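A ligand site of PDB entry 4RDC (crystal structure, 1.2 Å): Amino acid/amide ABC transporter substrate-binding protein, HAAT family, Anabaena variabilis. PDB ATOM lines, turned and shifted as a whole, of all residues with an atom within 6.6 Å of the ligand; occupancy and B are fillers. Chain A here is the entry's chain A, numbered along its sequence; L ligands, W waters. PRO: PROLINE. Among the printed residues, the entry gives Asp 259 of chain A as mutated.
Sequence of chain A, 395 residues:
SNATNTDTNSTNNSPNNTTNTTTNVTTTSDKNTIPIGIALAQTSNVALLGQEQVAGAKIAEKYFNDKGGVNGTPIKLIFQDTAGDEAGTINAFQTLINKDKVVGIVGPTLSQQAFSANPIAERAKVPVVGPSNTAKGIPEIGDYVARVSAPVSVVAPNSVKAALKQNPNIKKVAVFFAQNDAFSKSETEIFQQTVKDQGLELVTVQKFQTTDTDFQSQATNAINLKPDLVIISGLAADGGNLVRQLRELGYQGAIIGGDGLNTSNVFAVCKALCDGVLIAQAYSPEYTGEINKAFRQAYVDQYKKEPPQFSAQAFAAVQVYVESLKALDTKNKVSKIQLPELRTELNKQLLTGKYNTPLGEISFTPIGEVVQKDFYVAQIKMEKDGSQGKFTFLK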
ATOM      1  N   LEU A  49       4.433  33.294 -12.347  1.00  0.00           N
ATOM      2  CA  LEU A  49       3.203  32.958 -11.637  1.00  0.00           C
ATOM      3  C   LEU A  49       3.277  33.449 -10.188  1.00  0.00           C
ATOM      4  O   LEU A  49       2.344  34.078  -9.673  1.00  0.00           O
ATOM      5  CB  LEU A  49       2.959  31.443 -11.633  1.00  0.00           C
ATOM      6  CG  LEU A  49       2.640  30.730 -12.942  1.00  0.00           C
ATOM      7  CD1 LEU A  49       3.855  30.615 -13.846  1.00  0.00           C
ATOM      8  CD2 LEU A  49       2.070  29.353 -12.653  1.00  0.00           C
ATOM      9  N   GLN A  53       0.954  35.900  -6.948  1.00  0.00           N
ATOM     10  CA  GLN A  53       0.556  35.409  -5.648  1.00  0.00           C
ATOM     11  C   GLN A  53       1.096  36.288  -4.533  1.00  0.00           C
ATOM     12  O   GLN A  53       0.386  36.588  -3.577  1.00  0.00           O
ATOM     13  CB  GLN A  53       1.010  33.964  -5.488  1.00  0.00           C
ATOM     14  CG  GLN A  53       0.447  33.066  -6.564  1.00  0.00           C
ATOM     15  CD  GLN A  53       1.010  31.677  -6.459  1.00  0.00           C
ATOM     16  OE1 GLN A  53       2.226  31.475  -6.476  1.00  0.00           O
ATOM     17  NE2 GLN A  53       0.119  30.697  -6.346  1.00  0.00           N
ATOM     18  N   THR A 109       3.921  27.437  -4.907  1.00  0.00           N
ATOM     19  CA  THR A 109       3.306  27.803  -6.188  1.00  0.00           C
ATOM     20  C   THR A 109       2.948  26.584  -7.039  1.00  0.00           C
ATOM     21  O   THR A 109       1.842  26.511  -7.594  1.00  0.00           O
ATOM     22  CB  THR A 109       4.232  28.734  -6.966  1.00  0.00           C
ATOM     23  OG1 THR A 109       4.436  29.929  -6.199  1.00  0.00           O
ATOM     24  CG2 THR A 109       3.669  29.095  -8.331  1.00  0.00           C
ATOM     25  N   LEU A 110       3.846  25.615  -7.128  1.00  0.00           N
ATOM     26  CA  LEU A 110       3.640  24.483  -8.037  1.00  0.00           C
ATOM     27  C   LEU A 110       3.268  23.212  -7.300  1.00  0.00           C
ATOM     28  O   LEU A 110       3.818  22.914  -6.235  1.00  0.00           O
ATOM     29  CB  LEU A 110       4.913  24.212  -8.830  1.00  0.00           C
ATOM     30  CG  LEU A 110       5.423  25.316  -9.742  1.00  0.00           C
ATOM     31  CD1 LEU A 110       6.705  24.832 -10.435  1.00  0.00           C
ATOM     32  CD2 LEU A 110       4.370  25.750 -10.764  1.00  0.00           C
ATOM     33  N   SER A 111       2.379  22.419  -7.908  1.00  0.00           N
ATOM     34  CA  SER A 111       2.101  21.085  -7.394  1.00  0.00           C
ATOM     35  C   SER A 111       3.349  20.217  -7.302  1.00  0.00           C
ATOM     36  O   SER A 111       3.515  19.470  -6.342  1.00  0.00           O
ATOM     37  CB  SER A 111       1.055  20.370  -8.264  1.00  0.00           C
ATOM     38  OG  SER A 111      -0.211  21.004  -8.194  1.00  0.00           O
ATOM     39  N   GLN A 112       4.249  20.340  -8.280  1.00  0.00           N
ATOM     40  CA  GLN A 112       5.506  19.594  -8.255  1.00  0.00           C
ATOM     41  C   GLN A 112       6.248  19.870  -6.949  1.00  0.00           C
ATOM     42  O   GLN A 112       6.791  18.957  -6.317  1.00  0.00           O
ATOM     43  CB  GLN A 112       6.372  20.023  -9.443  1.00  0.00           C
ATOM     44  CG  GLN A 112       7.731  19.335  -9.548  1.00  0.00           C
ATOM     45  CD  GLN A 112       7.634  17.918 -10.084  1.00  0.00           C
ATOM     46  OE1 GLN A 112       6.781  17.596 -10.912  1.00  0.00           O
ATOM     47  NE2 GLN A 112       8.529  17.062  -9.617  1.00  0.00           N
ATOM     48  N   GLN A 113       6.266  21.136  -6.548  1.00  0.00           N
ATOM     49  CA  GLN A 113       6.919  21.548  -5.323  1.00  0.00           C
ATOM     50  C   GLN A 113       6.160  21.074  -4.088  1.00  0.00           C
ATOM     51  O   GLN A 113       6.768  20.653  -3.096  1.00  0.00           O
ATOM     52  CB  GLN A 113       7.083  23.070  -5.329  1.00  0.00           C
ATOM     53  CG  GLN A 113       8.067  23.542  -6.385  1.00  0.00           C
ATOM     54  CD  GLN A 113       8.071  25.051  -6.523  1.00  0.00           C
ATOM     55  OE1 GLN A 113       7.003  25.674  -6.611  1.00  0.00           O
ATOM     56  NE2 GLN A 113       9.259  25.650  -6.562  1.00  0.00           N
ATOM     57  N   SER A 132      -2.573  27.397  -5.402  1.00  0.00           N
ATOM     58  CA  SER A 132      -2.402  27.234  -6.849  1.00  0.00           C
ATOM     59  C   SER A 132      -1.883  25.853  -7.174  1.00  0.00           C
ATOM     60  O   SER A 132      -1.113  25.665  -8.129  1.00  0.00           O
ATOM     61  CB  SER A 132      -1.359  28.229  -7.376  1.00  0.00           C
ATOM     62  OG  SER A 132      -0.114  28.049  -6.708  1.00  0.00           O
ATOM     63  N   ASN A 133      -2.265  24.873  -6.374  1.00  0.00           N
ATOM     64  CA  ASN A 133      -1.774  23.532  -6.617  1.00  0.00           C
ATOM     65  C   ASN A 133      -2.948  22.707  -7.070  1.00  0.00           C
ATOM     66  O   ASN A 133      -3.754  22.261  -6.250  1.00  0.00           O
ATOM     67  CB  ASN A 133      -1.146  22.914  -5.360  1.00  0.00           C
ATOM     68  CG  ASN A 133      -0.166  23.842  -4.665  1.00  0.00           C
ATOM     69  OD1 ASN A 133      -0.143  23.906  -3.450  1.00  0.00           O
ATOM     70  ND2 ASN A 133       0.660  24.526  -5.434  1.00  0.00           N
ATOM     71  N   THR A 134      -3.054  22.500  -8.379  1.00  0.00           N
ATOM     72  CA  THR A 134      -4.283  21.975  -8.965  1.00  0.00           C
ATOM     73  C   THR A 134      -4.147  20.545  -9.500  1.00  0.00           C
ATOM     74  O   THR A 134      -5.102  19.991 -10.047  1.00  0.00           O
ATOM     75  CB  THR A 134      -4.798  22.930 -10.040  1.00  0.00           C
ATOM     76  OG1 THR A 134      -3.796  23.060 -11.076  1.00  0.00           O
ATOM     77  CG2 THR A 134      -5.076  24.295  -9.436  1.00  0.00           C
ATOM     78  N   ALA A 135      -2.987  19.933  -9.310  1.00  0.00           N
ATOM     79  CA  ALA A 135      -2.776  18.551  -9.715  1.00  0.00           C
ATOM     80  C   ALA A 135      -3.615  17.598  -8.897  1.00  0.00           C
ATOM     81  O   ALA A 135      -3.910  17.849  -7.727  1.00  0.00           O
ATOM     82  CB  ALA A 135      -1.317  18.174  -9.596  1.00  0.00           C
ATOM     83  N   ILE A 138      -3.224  16.401  -4.451  1.00  0.00           N
ATOM     84  CA  ILE A 138      -2.682  17.359  -3.494  1.00  0.00           C
ATOM     85  C   ILE A 138      -3.317  17.234  -2.092  1.00  0.00           C
ATOM     86  O   ILE A 138      -2.603  17.105  -1.115  1.00  0.00           O
ATOM     87  CB  ILE A 138      -2.736  18.807  -4.035  1.00  0.00           C
ATOM     88  CG1 ILE A 138      -1.745  18.984  -5.205  1.00  0.00           C
ATOM     89  CG2 ILE A 138      -2.440  19.811  -2.920  1.00  0.00           C
ATOM     90  CD1 ILE A 138      -0.276  19.011  -4.789  1.00  0.00           C
ATOM     91  N   SER A 149      -7.368  26.153  -4.352  1.00  0.00           N
ATOM     92  CA  SER A 149      -7.290  26.146  -5.802  1.00  0.00           C
ATOM     93  C   SER A 149      -8.000  24.928  -6.372  1.00  0.00           C
ATOM     94  O   SER A 149      -7.567  23.788  -6.166  1.00  0.00           O
ATOM     95  CB  SER A 149      -5.830  26.159  -6.246  1.00  0.00           C
ATOM     96  OG  SER A 149      -5.114  25.110  -5.640  1.00  0.00           O
ATOM     97  N   VAL A 152      -7.713  20.493 -11.573  1.00  0.00           N
ATOM     98  CA  VAL A 152      -7.740  20.471 -13.027  1.00  0.00           C
ATOM     99  C   VAL A 152      -9.002  19.809 -13.593  1.00  0.00           C
ATOM    100  O   VAL A 152      -9.538  20.262 -14.598  1.00  0.00           O
ATOM    101  CB  VAL A 152      -6.475  19.802 -13.628  1.00  0.00           C
ATOM    102  CG1 VAL A 152      -5.257  20.703 -13.429  1.00  0.00           C
ATOM    103  CG2 VAL A 152      -6.226  18.409 -13.048  1.00  0.00           C
ATOM    104  N   ASP A 181       6.724  18.014 -15.242  1.00  0.00           N
ATOM    105  CA  ASP A 181       5.967  18.767 -14.242  1.00  0.00           C
ATOM    106  C   ASP A 181       4.673  18.038 -13.832  1.00  0.00           C
ATOM    107  O   ASP A 181       3.853  17.685 -14.680  1.00  0.00           O
ATOM    108  CB  ASP A 181       5.643  20.150 -14.786  1.00  0.00           C
ATOM    109  CG  ASP A 181       4.808  20.956 -13.825  1.00  0.00           C
ATOM    110  OD1 ASP A 181       5.351  21.411 -12.797  1.00  0.00           O
ATOM    111  OD2 ASP A 181       3.603  21.130 -14.096  1.00  0.00           O
ATOM    112  N   ALA A 182       4.480  17.854 -12.522  1.00  0.00           N
ATOM    113  CA  ALA A 182       3.376  17.041 -12.009  1.00  0.00           C
ATOM    114  C   ALA A 182       2.013  17.605 -12.402  1.00  0.00           C
ATOM    115  O   ALA A 182       1.110  16.862 -12.804  1.00  0.00           O
ATOM    116  CB  ALA A 182       3.477  16.914 -10.500  1.00  0.00           C
ATOM    117  N   PHE A 183       1.843  18.917 -12.270  1.00  0.00           N
ATOM    118  CA  PHE A 183       0.603  19.560 -12.663  1.00  0.00           C
ATOM    119  C   PHE A 183       0.324  19.395 -14.156  1.00  0.00           C
ATOM    120  O   PHE A 183      -0.804  19.079 -14.544  1.00  0.00           O
ATOM    121  CB  PHE A 183       0.632  21.041 -12.289  1.00  0.00           C
ATOM    122  CG  PHE A 183      -0.126  21.927 -13.228  1.00  0.00           C
ATOM    123  CD1 PHE A 183      -1.515  21.980 -13.184  1.00  0.00           C
ATOM    124  CD2 PHE A 183       0.541  22.703 -14.158  1.00  0.00           C
ATOM    125  CE1 PHE A 183      -2.217  22.788 -14.052  1.00  0.00           C
ATOM    126  CE2 PHE A 183      -0.156  23.519 -15.029  1.00  0.00           C
ATOM    127  CZ  PHE A 183      -1.528  23.561 -14.981  1.00  0.00           C
ATOM    128  N   SER A 184       1.338  19.596 -14.983  1.00  0.00           N
ATOM    129  CA  SER A 184       1.141  19.520 -16.425  1.00  0.00           C
ATOM    130  C   SER A 184       0.697  18.127 -16.848  1.00  0.00           C
ATOM    131  O   SER A 184      -0.161  17.974 -17.717  1.00  0.00           O
ATOM    132  CB  SER A 184       2.427  19.933 -17.165  1.00  0.00           C
ATOM    133  OG  SER A 184       2.770  21.273 -16.871  1.00  0.00           O
ATOM    134  N   LEU A 235       4.067  25.695 -18.095  1.00  0.00           N
ATOM    135  CA  LEU A 235       4.070  26.909 -17.289  1.00  0.00           C
ATOM    136  C   LEU A 235       4.134  28.116 -18.233  1.00  0.00           C
ATOM    137  O   LEU A 235       3.822  27.985 -19.428  1.00  0.00           O
ATOM    138  CB  LEU A 235       5.171  26.874 -16.215  1.00  0.00           C
ATOM    139  CG  LEU A 235       5.049  25.670 -15.271  1.00  0.00           C
ATOM    140  CD1 LEU A 235       6.159  25.653 -14.235  1.00  0.00           C
ATOM    141  CD2 LEU A 235       3.675  25.616 -14.569  1.00  0.00           C
ATOM    142  N   ASP A 259      -3.671  26.141 -16.981  1.00  0.00           N
ATOM    143  CA  ASP A 259      -3.577  27.063 -15.854  1.00  0.00           C
ATOM    144  C   ASP A 259      -2.148  27.599 -15.638  1.00  0.00           C
ATOM    145  O   ASP A 259      -1.964  28.663 -15.046  1.00  0.00           O
ATOM    146  CB  ASP A 259      -4.092  26.365 -14.571  1.00  0.00           C
ATOM    147  CG  ASP A 259      -4.733  27.321 -13.562  1.00  0.00           C
ATOM    148  OD1 ASP A 259      -5.141  28.447 -13.924  1.00  0.00           O
ATOM    149  OD2 ASP A 259      -4.889  26.899 -12.398  1.00  0.00           O
ATOM    150  N   GLY A 260      -1.144  26.895 -16.148  1.00  0.00           N
ATOM    151  CA  GLY A 260       0.228  27.352 -16.009  1.00  0.00           C
ATOM    152  C   GLY A 260       0.534  28.579 -16.846  1.00  0.00           C
ATOM    153  O   GLY A 260       1.535  29.263 -16.615  1.00  0.00           O
ATOM    154  N   GLN A 309      -6.430  35.616 -11.503  1.00  0.00           N
ATOM    155  CA  GLN A 309      -6.772  34.460 -10.681  1.00  0.00           C
ATOM    156  C   GLN A 309      -5.787  34.164  -9.560  1.00  0.00           C
ATOM    157  O   GLN A 309      -6.173  33.938  -8.423  1.00  0.00           O
ATOM    158  CB  GLN A 309      -6.915  33.227 -11.563  1.00  0.00           C
ATOM    159  CG  GLN A 309      -7.281  31.986 -10.773  1.00  0.00           C
ATOM    160  CD  GLN A 309      -7.159  30.746 -11.614  1.00  0.00           C
ATOM    161  OE1 GLN A 309      -7.976  30.485 -12.486  1.00  0.00           O
ATOM    162  NE2 GLN A 309      -6.100  29.992 -11.380  1.00  0.00           N
ATOM    163  N   PHE A 310      -4.496  34.125  -9.886  1.00  0.00           N
ATOM    164  CA  PHE A 310      -3.538  33.689  -8.883  1.00  0.00           C
ATOM    165  C   PHE A 310      -3.461  34.658  -7.698  1.00  0.00           C
ATOM    166  O   PHE A 310      -3.218  34.249  -6.556  1.00  0.00           O
ATOM    167  CB  PHE A 310      -2.143  33.469  -9.484  1.00  0.00           C
ATOM    168  CG  PHE A 310      -2.067  32.309 -10.439  1.00  0.00           C
ATOM    169  CD1 PHE A 310      -2.712  31.111 -10.163  1.00  0.00           C
ATOM    170  CD2 PHE A 310      -1.349  32.400 -11.605  1.00  0.00           C
ATOM    171  CE1 PHE A 310      -2.653  30.043 -11.045  1.00  0.00           C
ATOM    172  CE2 PHE A 310      -1.285  31.340 -12.491  1.00  0.00           C
ATOM    173  CZ  PHE A 310      -1.941  30.167 -12.203  1.00  0.00           C
ATOM    174  N   GLN A 313      -6.586  33.903  -5.596  1.00  0.00           N
ATOM    175  CA  GLN A 313      -6.437  32.653  -4.864  1.00  0.00           C
ATOM    176  C   GLN A 313      -5.485  32.782  -3.677  1.00  0.00           C
ATOM    177  O   GLN A 313      -5.742  32.243  -2.607  1.00  0.00           O
ATOM    178  CB  GLN A 313      -6.030  31.508  -5.798  1.00  0.00           C
ATOM    179  CG  GLN A 313      -7.146  31.108  -6.752  1.00  0.00           C
ATOM    180  CD  GLN A 313      -6.711  30.058  -7.754  1.00  0.00           C
ATOM    181  OE1 GLN A 313      -5.601  30.130  -8.300  1.00  0.00           O
ATOM    182  NE2 GLN A 313      -7.585  29.085  -8.029  1.00  0.00           N
HETATM  183  N   PRO L   1      -1.645  25.079 -10.988  1.00  0.00           N
HETATM  184  CA  PRO L   1      -0.265  24.768 -11.351  1.00  0.00           C
HETATM  185  C   PRO L   1       0.249  23.707 -10.418  1.00  0.00           C
HETATM  186  O   PRO L   1       1.473  23.480 -10.384  1.00  0.00           O
HETATM  187  CB  PRO L   1       0.456  26.096 -11.112  1.00  0.00           C
HETATM  188  CG  PRO L   1      -0.593  27.120 -11.436  1.00  0.00           C
HETATM  189  CD  PRO L   1      -1.966  26.479 -11.282  1.00  0.00           C
HETATM  190  OXT PRO L   1      -0.557  23.084  -9.724  1.00  0.00           O
HETATM  191  O   HOH W   1       3.560  21.500 -10.796  1.00  0.00           O
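The side-chain carboxylate of Asp 259 is in salt-bridge range of a nitrogen (N) of the ligand. N of Thr 134 lies within hydrogen-bond range of OXT of the ligand, at 2.9 Å. O of Ser 132 lies within hydrogen-bond range of N of the ligand (3.0 Å). N of Ser 111 lies within hydrogen-bond range of O of the ligand, 2.8 Å away. OG of Ser 111 lies within hydrogen-bond range of OXT of the ligand (2.6 Å). The side-chain hydroxyl (OG1) of Thr 134 lies within hydrogen-bond range of a nitrogen (N) of the ligand.
The backbone NH of Phe 183 lies close to the side-chain carboxylate of Asp 181 (3.4 Å). The backbone NH (N) of Ala 135 sits at hydrogen-bond distance from the side-chain hydroxyl (OG) of Ser 111 (3.2 Å). O of Thr 109 sits at hydrogen-bond distance from OG of Ser 132 (2.6 Å). The side-chain amide nitrogen of Gln 309 sits at hydrogen-bond distance from the side-chain carboxylate of Asp 259, at 3.1 Å. The backbone NH (N) of Leu 110 sits at hydrogen-bond distance from the side-chain amide oxygen (OE1) of Gln 113 (3.2 Å). The side-chain amide nitrogen of Asn 133 is in hydrogen-bond range of the backbone carbonyl oxygen of Thr 109 (3.2 Å). The side-chain hydroxyl of Thr 109 is in hydrogen-bond range of the side-chain amide oxygen of Gln 53, 2.7 Å away. N of Val 152 sits at hydrogen-bond distance from O of Thr 134 (3.1 Å).
Residues that only touch the ligand: Leu 49, Thr 109, Leu 110, Asn 133, Phe 183 and Phe 310. Hydrophobic or aromatic side chains that line the ligand: Leu 49, Leu 110, Phe 183 and Phe 310. Of the 24 residues printed, 10 come within 4 Å of the ligand. The nearest printed residue that does not touch the ligand is Ala 135 (4.001 Å).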
